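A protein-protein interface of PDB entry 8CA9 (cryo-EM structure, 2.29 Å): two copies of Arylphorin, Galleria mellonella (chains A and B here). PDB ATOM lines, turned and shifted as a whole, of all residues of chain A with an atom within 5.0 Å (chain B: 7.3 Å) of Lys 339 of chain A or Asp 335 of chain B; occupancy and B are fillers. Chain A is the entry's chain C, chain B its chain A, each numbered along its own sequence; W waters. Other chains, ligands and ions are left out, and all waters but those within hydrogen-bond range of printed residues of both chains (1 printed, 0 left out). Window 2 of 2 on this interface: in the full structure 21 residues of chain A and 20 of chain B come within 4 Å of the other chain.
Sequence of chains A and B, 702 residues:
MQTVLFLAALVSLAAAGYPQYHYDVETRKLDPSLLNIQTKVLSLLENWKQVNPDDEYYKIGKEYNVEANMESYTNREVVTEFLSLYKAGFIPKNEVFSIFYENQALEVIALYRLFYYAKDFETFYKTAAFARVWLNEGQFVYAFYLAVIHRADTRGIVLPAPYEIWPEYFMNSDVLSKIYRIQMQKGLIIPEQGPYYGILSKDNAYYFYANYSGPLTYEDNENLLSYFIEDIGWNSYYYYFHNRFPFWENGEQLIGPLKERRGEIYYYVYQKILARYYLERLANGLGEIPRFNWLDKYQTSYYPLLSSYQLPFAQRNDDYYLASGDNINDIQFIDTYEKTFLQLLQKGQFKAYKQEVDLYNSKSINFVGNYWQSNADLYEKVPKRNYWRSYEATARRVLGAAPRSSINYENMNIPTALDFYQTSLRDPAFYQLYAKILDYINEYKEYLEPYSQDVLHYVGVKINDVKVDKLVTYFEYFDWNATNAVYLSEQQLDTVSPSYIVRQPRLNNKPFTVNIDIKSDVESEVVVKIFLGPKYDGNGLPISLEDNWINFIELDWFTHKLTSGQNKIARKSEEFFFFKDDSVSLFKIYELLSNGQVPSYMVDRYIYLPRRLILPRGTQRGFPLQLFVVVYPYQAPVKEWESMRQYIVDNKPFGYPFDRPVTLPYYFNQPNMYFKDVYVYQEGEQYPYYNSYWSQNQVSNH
Printed residues of chain A that touch a printed residue of chain B: Asp 335, Glu 338, Lys 339, Leu 342 and Gln 343.
Hydrophobic or aromatic side chains of chain A within 4 Å of the printed part of chain B: Leu 342.
Among the printed residues, 8 pairs touch across the chains.
Among the printed residues, Asp or Glu carboxylates within 4 Å of a Lys or Arg side-chain nitrogen of the other chain: Lys 339 of chain A with Asp 335 of chain B (3.0 Å).
Lys 339 of chain A touches three residues of chain B.
Asp 335 of chain B touches just one residue of chain A: Lys 339 (3.0 Å).
Of the printed residues of chain B, Asp 335 of chain A touches Gln 332 (3.5 Å).
Of the printed residues of chain A, Thr 336 of chain B touches Lys 339 (3.5 Å), Leu 342 (3.2 Å) and Gln 343 (3.99 Å).
Of the printed residues of chain A, Thr 340 of chain B touches Gln 343 (3.5 Å).
Of the printed residues of chain B, Leu 342 of chain A touches Thr 336.
The nearest residue of chain B that does not touch Lys 339 of chain A is Lys 339 of chain B (4.9 Å).
The nearest residue of chain A that does not touch Asp 335 of chain B is Asp 335 of chain A (4.9 Å).
The side-chain carboxylate (OD2) of Asp 335 of chain B is in salt-bridge range of the side-chain amino group (NZ) of Lys 339 of chain A (3.0 Å).
The side-chain carboxylate of Glu 338 of chain A is in hydrogen-bond range of the side-chain amide nitrogen of Gln 332 of chain B (3.0 Å).
The side-chain hydroxyl (OG1) of Thr 340 of chain B sits at hydrogen-bond distance from the side-chain amide nitrogen (NE2) of Gln 343 of chain A (3.5 Å).
The side-chain amide nitrogen of Gln 332 of chain B is in hydrogen-bond range of the side-chain carboxylate of Asp 335 of chain A, 3.5 Å away.
Water W1 bridges the side-chain carboxylate (OD1) of Asp 335 of chain A and the side-chain amide nitrogen (NE2) of Gln 332 of chain B.
Lys 339 of chain A touches Asp 335 of chain B, but with the chains exchanged Asp 335 of chain A does not touch Lys 339 of chain B (5.8 Å).
Lys 339 of chain A touches Thr 336 of chain B, but with the chains exchanged Thr 336 of chain A does not touch Lys 339 of chain B (8.5 Å).
Of the 8 pairs that touch across the chains among the printed residues, none has its exchanged pair printed and touching as well.
Among the printed residues, merely in contact across the chains: Lys 339 of chain A with Gln 332 of chain B, Lys 339 of chain A with Thr 336 of chain B, Leu 342 of chain A with Thr 336 of chain B and Gln 343 of chain A with Thr 336 of chain B.
OD1 of Asp 335 of chain B is in salt-bridge range of NZ of Lys 339 of chain B (2.8 Å).
The side-chain hydroxyl (OG1) of Thr 336 of chain B is in hydrogen-bond range of the backbone carbonyl oxygen (O) of Gln 332 of chain B (3.0 Å).
The side-chain hydroxyl (OG1) of Thr 340 of chain B is in hydrogen-bond range of the backbone carbonyl oxygen (O) of Thr 336 of chain B (3.2 Å).
The side-chain carboxylate (OD1) of Asp 335 of chain A lies within salt-bridge range of the side-chain amino group (NZ) of Lys 339 of chain A (2.8 Å).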
ATOM      1  N   ASP A 335      -2.075  -6.613  -3.564  1.00  0.00           N
ATOM      2  CA  ASP A 335      -0.670  -6.569  -3.942  1.00  0.00           C
ATOM      3  C   ASP A 335       0.044  -7.817  -3.449  1.00  0.00           C
ATOM      4  O   ASP A 335       0.671  -8.542  -4.233  1.00  0.00           O
ATOM      5  CB  ASP A 335      -0.013  -5.309  -3.376  1.00  0.00           C
ATOM      6  CG  ASP A 335       1.330  -5.013  -4.014  1.00  0.00           C
ATOM      7  OD1 ASP A 335       1.694  -5.705  -4.989  1.00  0.00           O
ATOM      8  OD2 ASP A 335       2.022  -4.088  -3.541  1.00  0.00           O
ATOM      9  N   THR A 336      -0.111  -8.127  -2.160  1.00  0.00           N
ATOM     10  CA  THR A 336       0.586  -9.276  -1.598  1.00  0.00           C
ATOM     11  C   THR A 336       0.308 -10.514  -2.432  1.00  0.00           C
ATOM     12  O   THR A 336       1.235 -11.202  -2.878  1.00  0.00           O
ATOM     13  CB  THR A 336       0.161  -9.493  -0.145  1.00  0.00           C
ATOM     14  OG1 THR A 336       0.355  -8.283   0.600  1.00  0.00           O
ATOM     15  CG2 THR A 336       0.978 -10.608   0.492  1.00  0.00           C
ATOM     16  N   TYR A 337      -0.973 -10.773  -2.710  1.00  0.00           N
ATOM     17  CA  TYR A 337      -1.329 -11.939  -3.507  1.00  0.00           C
ATOM     18  C   TYR A 337      -0.484 -11.985  -4.772  1.00  0.00           C
ATOM     19  O   TYR A 337       0.266 -12.943  -5.001  1.00  0.00           O
ATOM     20  CB  TYR A 337      -2.821 -11.902  -3.843  1.00  0.00           C
ATOM     21  CG  TYR A 337      -3.487 -13.260  -3.879  1.00  0.00           C
ATOM     22  CD1 TYR A 337      -3.792 -13.936  -2.705  1.00  0.00           C
ATOM     23  CD2 TYR A 337      -3.828 -13.857  -5.084  1.00  0.00           C
ATOM     24  CE1 TYR A 337      -4.406 -15.173  -2.731  1.00  0.00           C
ATOM     25  CE2 TYR A 337      -4.443 -15.094  -5.120  1.00  0.00           C
ATOM     26  CZ  TYR A 337      -4.730 -15.747  -3.941  1.00  0.00           C
ATOM     27  OH  TYR A 337      -5.342 -16.978  -3.970  1.00  0.00           O
ATOM     28  N   GLU A 338      -0.531 -10.912  -5.565  1.00  0.00           N
ATOM     29  CA  GLU A 338       0.239 -10.885  -6.803  1.00  0.00           C
ATOM     30  C   GLU A 338       1.703 -11.188  -6.523  1.00  0.00           C
ATOM     31  O   GLU A 338       2.290 -12.093  -7.131  1.00  0.00           O
ATOM     32  CB  GLU A 338       0.087  -9.525  -7.484  1.00  0.00           C
ATOM     33  CG  GLU A 338      -1.341  -9.182  -7.878  1.00  0.00           C
ATOM     34  CD  GLU A 338      -1.452  -7.820  -8.535  1.00  0.00           C
ATOM     35  OE1 GLU A 338      -0.407  -7.161  -8.720  1.00  0.00           O
ATOM     36  OE2 GLU A 338      -2.583  -7.408  -8.867  1.00  0.00           O
ATOM     37  N   LYS A 339       2.291 -10.481  -5.554  1.00  0.00           N
ATOM     38  CA  LYS A 339       3.696 -10.699  -5.236  1.00  0.00           C
ATOM     39  C   LYS A 339       3.962 -12.178  -5.014  1.00  0.00           C
ATOM     40  O   LYS A 339       4.879 -12.758  -5.608  1.00  0.00           O
ATOM     41  CB  LYS A 339       4.089  -9.898  -3.994  1.00  0.00           C
ATOM     42  CG  LYS A 339       4.981  -8.702  -4.269  1.00  0.00           C
ATOM     43  CD  LYS A 339       4.190  -7.491  -4.720  1.00  0.00           C
ATOM     44  CE  LYS A 339       5.109  -6.304  -4.945  1.00  0.00           C
ATOM     45  NZ  LYS A 339       4.369  -5.035  -5.168  1.00  0.00           N
ATOM     46  N   THR A 340       3.123 -12.818  -4.195  1.00  0.00           N
ATOM     47  CA  THR A 340       3.347 -14.219  -3.873  1.00  0.00           C
ATOM     48  C   THR A 340       3.484 -15.046  -5.141  1.00  0.00           C
ATOM     49  O   THR A 340       4.447 -15.809  -5.294  1.00  0.00           O
ATOM     50  CB  THR A 340       2.204 -14.737  -2.999  1.00  0.00           C
ATOM     51  OG1 THR A 340       2.188 -14.021  -1.757  1.00  0.00           O
ATOM     52  CG2 THR A 340       2.361 -16.220  -2.718  1.00  0.00           C
ATOM     53  N   PHE A 341       2.570 -14.855  -6.097  1.00  0.00           N
ATOM     54  CA  PHE A 341       2.621 -15.656  -7.312  1.00  0.00           C
ATOM     55  C   PHE A 341       3.961 -15.487  -8.011  1.00  0.00           C
ATOM     56  O   PHE A 341       4.590 -16.473  -8.413  1.00  0.00           O
ATOM     57  CB  PHE A 341       1.473 -15.275  -8.247  1.00  0.00           C
ATOM     58  CG  PHE A 341       1.308 -16.210  -9.411  1.00  0.00           C
ATOM     59  CD1 PHE A 341       0.732 -17.456  -9.237  1.00  0.00           C
ATOM     60  CD2 PHE A 341       1.728 -15.843 -10.679  1.00  0.00           C
ATOM     61  CE1 PHE A 341       0.578 -18.320 -10.303  1.00  0.00           C
ATOM     62  CE2 PHE A 341       1.575 -16.704 -11.749  1.00  0.00           C
ATOM     63  CZ  PHE A 341       1.000 -17.943 -11.561  1.00  0.00           C
ATOM     64  N   LEU A 342       4.438 -14.244  -8.124  1.00  0.00           N
ATOM     65  CA  LEU A 342       5.721 -14.022  -8.778  1.00  0.00           C
ATOM     66  C   LEU A 342       6.825 -14.785  -8.063  1.00  0.00           C
ATOM     67  O   LEU A 342       7.663 -15.430  -8.706  1.00  0.00           O
ATOM     68  CB  LEU A 342       6.036 -12.527  -8.828  1.00  0.00           C
ATOM     69  CG  LEU A 342       5.105 -11.673  -9.691  1.00  0.00           C
ATOM     70  CD1 LEU A 342       5.481 -10.202  -9.596  1.00  0.00           C
ATOM     71  CD2 LEU A 342       5.128 -12.137 -11.139  1.00  0.00           C
ATOM     72  N   GLN A 343       6.816 -14.765  -6.728  1.00  0.00           N
ATOM     73  CA  GLN A 343       7.819 -15.520  -5.988  1.00  0.00           C
ATOM     74  C   GLN A 343       7.754 -16.994  -6.355  1.00  0.00           C
ATOM     75  O   GLN A 343       8.791 -17.639  -6.557  1.00  0.00           O
ATOM     76  CB  GLN A 343       7.622 -15.326  -4.485  1.00  0.00           C
ATOM     77  CG  GLN A 343       7.960 -13.929  -3.991  1.00  0.00           C
ATOM     78  CD  GLN A 343       7.776 -13.778  -2.495  1.00  0.00           C
ATOM     79  OE1 GLN A 343       7.064 -14.558  -1.864  1.00  0.00           O
ATOM     80  NE2 GLN A 343       8.423 -12.773  -1.917  1.00  0.00           N
ATOM     81  N   TRP B 294      10.685   3.959  -7.285  1.00  0.00           N
ATOM     82  CA  TRP B 294      10.162   3.456  -8.553  1.00  0.00           C
ATOM     83  C   TRP B 294       8.763   3.985  -8.838  1.00  0.00           C
ATOM     84  O   TRP B 294       8.438   4.282  -9.993  1.00  0.00           O
ATOM     85  CB  TRP B 294      10.150   1.928  -8.548  1.00  0.00           C
ATOM     86  CG  TRP B 294      11.504   1.304  -8.680  1.00  0.00           C
ATOM     87  CD1 TRP B 294      12.218   0.682  -7.699  1.00  0.00           C
ATOM     88  CD2 TRP B 294      12.309   1.240  -9.864  1.00  0.00           C
ATOM     89  NE1 TRP B 294      13.417   0.234  -8.198  1.00  0.00           N
ATOM     90  CE2 TRP B 294      13.497   0.565  -9.524  1.00  0.00           C
ATOM     91  CE3 TRP B 294      12.139   1.689 -11.177  1.00  0.00           C
ATOM     92  CZ2 TRP B 294      14.510   0.328 -10.449  1.00  0.00           C
ATOM     93  CZ3 TRP B 294      13.147   1.452 -12.093  1.00  0.00           C
ATOM     94  CH2 TRP B 294      14.317   0.777 -11.725  1.00  0.00           C
ATOM     95  N   LEU B 295       7.925   4.109  -7.811  1.00  0.00           N
ATOM     96  CA  LEU B 295       6.540   4.527  -7.978  1.00  0.00           C
ATOM     97  C   LEU B 295       6.371   6.044  -7.940  1.00  0.00           C
ATOM     98  O   LEU B 295       5.277   6.527  -7.628  1.00  0.00           O
ATOM     99  CB  LEU B 295       5.664   3.874  -6.907  1.00  0.00           C
ATOM    100  CG  LEU B 295       5.679   2.343  -6.875  1.00  0.00           C
ATOM    101  CD1 LEU B 295       4.931   1.826  -5.655  1.00  0.00           C
ATOM    102  CD2 LEU B 295       5.085   1.769  -8.151  1.00  0.00           C
ATOM    103  N   ASN B 329       3.642  -4.230 -15.230  1.00  0.00           N
ATOM    104  CA  ASN B 329       4.145  -5.579 -15.009  1.00  0.00           C
ATOM    105  C   ASN B 329       5.614  -5.544 -14.610  1.00  0.00           C
ATOM    106  O   ASN B 329       5.993  -6.015 -13.530  1.00  0.00           O
ATOM    107  CB  ASN B 329       3.944  -6.425 -16.268  1.00  0.00           C
ATOM    108  CG  ASN B 329       2.484  -6.714 -16.550  1.00  0.00           C
ATOM    109  OD1 ASN B 329       1.651  -6.702 -15.643  1.00  0.00           O
ATOM    110  ND2 ASN B 329       2.166  -6.980 -17.810  1.00  0.00           N
ATOM    111  N   ASP B 330       6.452  -4.939 -15.456  1.00  0.00           N
ATOM    112  CA  ASP B 330       7.873  -4.854 -15.145  1.00  0.00           C
ATOM    113  C   ASP B 330       8.081  -4.294 -13.747  1.00  0.00           C
ATOM    114  O   ASP B 330       8.769  -4.901 -12.917  1.00  0.00           O
ATOM    115  CB  ASP B 330       8.585  -3.987 -16.186  1.00  0.00           C
ATOM    116  CG  ASP B 330       8.729  -4.681 -17.526  1.00  0.00           C
ATOM    117  OD1 ASP B 330       8.300  -5.849 -17.644  1.00  0.00           O
ATOM    118  OD2 ASP B 330       9.272  -4.059 -18.462  1.00  0.00           O
ATOM    119  N   ILE B 331       7.436  -3.162 -13.451  1.00  0.00           N
ATOM    120  CA  ILE B 331       7.587  -2.549 -12.134  1.00  0.00           C
ATOM    121  C   ILE B 331       7.357  -3.592 -11.052  1.00  0.00           C
ATOM    122  O   ILE B 331       8.209  -3.809 -10.180  1.00  0.00           O
ATOM    123  CB  ILE B 331       6.625  -1.355 -11.982  1.00  0.00           C
ATOM    124  CG1 ILE B 331       7.019  -0.220 -12.934  1.00  0.00           C
ATOM    125  CG2 ILE B 331       6.601  -0.864 -10.541  1.00  0.00           C
ATOM    126  CD1 ILE B 331       8.344   0.447 -12.608  1.00  0.00           C
ATOM    127  N   GLN B 332       6.231  -4.304 -11.137  1.00  0.00           N
ATOM    128  CA  GLN B 332       5.917  -5.293 -10.114  1.00  0.00           C
ATOM    129  C   GLN B 332       7.086  -6.247  -9.926  1.00  0.00           C
ATOM    130  O   GLN B 332       7.610  -6.397  -8.814  1.00  0.00           O
ATOM    131  CB  GLN B 332       4.649  -6.060 -10.491  1.00  0.00           C
ATOM    132  CG  GLN B 332       3.377  -5.229 -10.447  1.00  0.00           C
ATOM    133  CD  GLN B 332       3.020  -4.777  -9.045  1.00  0.00           C
ATOM    134  OE1 GLN B 332       3.604  -3.830  -8.517  1.00  0.00           O
ATOM    135  NE2 GLN B 332       2.057  -5.455  -8.432  1.00  0.00           N
ATOM    136  N   PHE B 333       7.564  -6.837 -11.025  1.00  0.00           N
ATOM    137  CA  PHE B 333       8.676  -7.770 -10.919  1.00  0.00           C
ATOM    138  C   PHE B 333       9.824  -7.127 -10.159  1.00  0.00           C
ATOM    139  O   PHE B 333      10.284  -7.656  -9.138  1.00  0.00           O
ATOM    140  CB  PHE B 333       9.124  -8.213 -12.315  1.00  0.00           C
ATOM    141  CG  PHE B 333      10.368  -9.055 -12.317  1.00  0.00           C
ATOM    142  CD1 PHE B 333      10.298 -10.425 -12.129  1.00  0.00           C
ATOM    143  CD2 PHE B 333      11.609  -8.475 -12.518  1.00  0.00           C
ATOM    144  CE1 PHE B 333      11.444 -11.198 -12.134  1.00  0.00           C
ATOM    145  CE2 PHE B 333      12.757  -9.244 -12.524  1.00  0.00           C
ATOM    146  CZ  PHE B 333      12.674 -10.607 -12.332  1.00  0.00           C
ATOM    147  N   ILE B 334      10.239  -5.933 -10.595  1.00  0.00           N
ATOM    148  CA  ILE B 334      11.311  -5.224  -9.904  1.00  0.00           C
ATOM    149  C   ILE B 334      11.028  -5.210  -8.410  1.00  0.00           C
ATOM    150  O   ILE B 334      11.786  -5.770  -7.606  1.00  0.00           O
ATOM    151  CB  ILE B 334      11.466  -3.800 -10.466  1.00  0.00           C
ATOM    152  CG1 ILE B 334      12.120  -3.848 -11.849  1.00  0.00           C
ATOM    153  CG2 ILE B 334      12.268  -2.925  -9.507  1.00  0.00           C
ATOM    154  CD1 ILE B 334      12.078  -2.531 -12.599  1.00  0.00           C
ATOM    155  N   ASP B 335       9.882  -4.642  -8.030  1.00  0.00           N
ATOM    156  CA  ASP B 335       9.555  -4.542  -6.615  1.00  0.00           C
ATOM    157  C   ASP B 335       9.669  -5.906  -5.953  1.00  0.00           C
ATOM    158  O   ASP B 335      10.394  -6.073  -4.964  1.00  0.00           O
ATOM    159  CB  ASP B 335       8.148  -3.970  -6.442  1.00  0.00           C
ATOM    160  CG  ASP B 335       7.876  -3.506  -5.023  1.00  0.00           C
ATOM    161  OD1 ASP B 335       8.820  -3.502  -4.204  1.00  0.00           O
ATOM    162  OD2 ASP B 335       6.718  -3.145  -4.727  1.00  0.00           O
ATOM    163  N   THR B 336       9.018  -6.913  -6.540  1.00  0.00           N
ATOM    164  CA  THR B 336       9.030  -8.238  -5.937  1.00  0.00           C
ATOM    165  C   THR B 336      10.460  -8.675  -5.667  1.00  0.00           C
ATOM    166  O   THR B 336      10.807  -9.053  -4.541  1.00  0.00           O
ATOM    167  CB  THR B 336       8.318  -9.241  -6.846  1.00  0.00           C
ATOM    168  OG1 THR B 336       7.003  -8.762  -7.154  1.00  0.00           O
ATOM    169  CG2 THR B 336       8.211 -10.600  -6.168  1.00  0.00           C
ATOM    170  N   TYR B 337      11.322  -8.562  -6.681  1.00  0.00           N
ATOM    171  CA  TYR B 337      12.714  -8.954  -6.507  1.00  0.00           C
ATOM    172  C   TYR B 337      13.281  -8.322  -5.246  1.00  0.00           C
ATOM    173  O   TYR B 337      13.711  -9.024  -4.321  1.00  0.00           O
ATOM    174  CB  TYR B 337      13.525  -8.550  -7.740  1.00  0.00           C
ATOM    175  CG  TYR B 337      14.625  -9.518  -8.111  1.00  0.00           C
ATOM    176  CD1 TYR B 337      14.333 -10.727  -8.730  1.00  0.00           C
ATOM    177  CD2 TYR B 337      15.957  -9.219  -7.859  1.00  0.00           C
ATOM    178  CE1 TYR B 337      15.334 -11.613  -9.076  1.00  0.00           C
ATOM    179  CE2 TYR B 337      16.964 -10.098  -8.203  1.00  0.00           C
ATOM    180  CZ  TYR B 337      16.648 -11.293  -8.812  1.00  0.00           C
ATOM    181  OH  TYR B 337      17.648 -12.174  -9.156  1.00  0.00           O
ATOM    182  N   GLU B 338      13.214  -6.992  -5.157  1.00  0.00           N
ATOM    183  CA  GLU B 338      13.749  -6.310  -3.986  1.00  0.00           C
ATOM    184  C   GLU B 338      13.148  -6.888  -2.715  1.00  0.00           C
ATOM    185  O   GLU B 338      13.874  -7.300  -1.799  1.00  0.00           O
ATOM    186  CB  GLU B 338      13.477  -4.810  -4.082  1.00  0.00           C
ATOM    187  CG  GLU B 338      14.119  -4.135  -5.283  1.00  0.00           C
ATOM    188  CD  GLU B 338      13.811  -2.653  -5.353  1.00  0.00           C
ATOM    189  OE1 GLU B 338      13.128  -2.142  -4.440  1.00  0.00           O
ATOM    190  OE2 GLU B 338      14.250  -1.995  -6.320  1.00  0.00           O
ATOM    191  N   LYS B 339      11.817  -6.987  -2.668  1.00  0.00           N
ATOM    192  CA  LYS B 339      11.160  -7.515  -1.479  1.00  0.00           C
ATOM    193  C   LYS B 339      11.780  -8.844  -1.083  1.00  0.00           C
ATOM    194  O   LYS B 339      12.171  -9.047   0.073  1.00  0.00           O
ATOM    195  CB  LYS B 339       9.662  -7.682  -1.730  1.00  0.00           C
ATOM    196  CG  LYS B 339       8.783  -6.679  -1.008  1.00  0.00           C
ATOM    197  CD  LYS B 339       8.693  -5.360  -1.752  1.00  0.00           C
ATOM    198  CE  LYS B 339       7.775  -4.397  -1.021  1.00  0.00           C
ATOM    199  NZ  LYS B 339       7.471  -3.178  -1.815  1.00  0.00           N
ATOM    200  N   THR B 340      11.928  -9.746  -2.056  1.00  0.00           N
ATOM    201  CA  THR B 340      12.447 -11.071  -1.749  1.00  0.00           C
ATOM    202  C   THR B 340      13.768 -10.968  -1.001  1.00  0.00           C
ATOM    203  O   THR B 340      13.941 -11.589   0.057  1.00  0.00           O
ATOM    204  CB  THR B 340      12.607 -11.874  -3.040  1.00  0.00           C
ATOM    205  OG1 THR B 340      11.322 -12.062  -3.649  1.00  0.00           O
ATOM    206  CG2 THR B 340      13.230 -13.230  -2.764  1.00  0.00           C
ATOM    207  N   PHE B 341      14.685 -10.133  -1.494  1.00  0.00           N
ATOM    208  CA  PHE B 341      15.988 -10.032  -0.850  1.00  0.00           C
ATOM    209  C   PHE B 341      15.835  -9.631   0.609  1.00  0.00           C
ATOM    210  O   PHE B 341      16.449 -10.237   1.496  1.00  0.00           O
ATOM    211  CB  PHE B 341      16.872  -9.033  -1.594  1.00  0.00           C
ATOM    212  CG  PHE B 341      18.306  -9.044  -1.144  1.00  0.00           C
ATOM    213  CD1 PHE B 341      19.158 -10.063  -1.532  1.00  0.00           C
ATOM    214  CD2 PHE B 341      18.802  -8.036  -0.334  1.00  0.00           C
ATOM    215  CE1 PHE B 341      20.476 -10.079  -1.121  1.00  0.00           C
ATOM    216  CE2 PHE B 341      20.120  -8.047   0.080  1.00  0.00           C
ATOM    217  CZ  PHE B 341      20.957  -9.069  -0.315  1.00  0.00           C
ATOM    218  N   TYR B 391      16.640  -8.693 -13.275  1.00  0.00           N
ATOM    219  CA  TYR B 391      16.353  -7.431 -12.601  1.00  0.00           C
ATOM    220  C   TYR B 391      17.039  -6.267 -13.306  1.00  0.00           C
ATOM    221  O   TYR B 391      16.423  -5.224 -13.553  1.00  0.00           O
ATOM    222  CB  TYR B 391      16.798  -7.517 -11.139  1.00  0.00           C
ATOM    223  CG  TYR B 391      16.652  -6.230 -10.359  1.00  0.00           C
ATOM    224  CD1 TYR B 391      15.495  -5.955  -9.647  1.00  0.00           C
ATOM    225  CD2 TYR B 391      17.678  -5.295 -10.327  1.00  0.00           C
ATOM    226  CE1 TYR B 391      15.361  -4.783  -8.930  1.00  0.00           C
ATOM    227  CE2 TYR B 391      17.552  -4.121  -9.615  1.00  0.00           C
ATOM    228  CZ  TYR B 391      16.392  -3.869  -8.917  1.00  0.00           C
ATOM    229  OH  TYR B 391      16.261  -2.700  -8.204  1.00  0.00           O
ATOM    230  N   TYR B 440      21.542  -2.238  -1.027  1.00  0.00           N
ATOM    231  CA  TYR B 440      21.028  -3.537  -0.590  1.00  0.00           C
ATOM    232  C   TYR B 440      22.171  -4.468  -0.194  1.00  0.00           C
ATOM    233  O   TYR B 440      22.107  -5.158   0.834  1.00  0.00           O
ATOM    234  CB  TYR B 440      20.180  -4.178  -1.689  1.00  0.00           C
ATOM    235  CG  TYR B 440      18.808  -3.569  -1.864  1.00  0.00           C
ATOM    236  CD1 TYR B 440      17.850  -3.662  -0.861  1.00  0.00           C
ATOM    237  CD2 TYR B 440      18.462  -2.922  -3.039  1.00  0.00           C
ATOM    238  CE1 TYR B 440      16.592  -3.112  -1.023  1.00  0.00           C
ATOM    239  CE2 TYR B 440      17.209  -2.372  -3.210  1.00  0.00           C
ATOM    240  CZ  TYR B 440      16.278  -2.469  -2.201  1.00  0.00           C
ATOM    241  OH  TYR B 440      15.030  -1.918  -2.375  1.00  0.00           O
HETATM  242  O   HOH W   1      -0.257  -3.697  -6.594  1.00  0.00           O
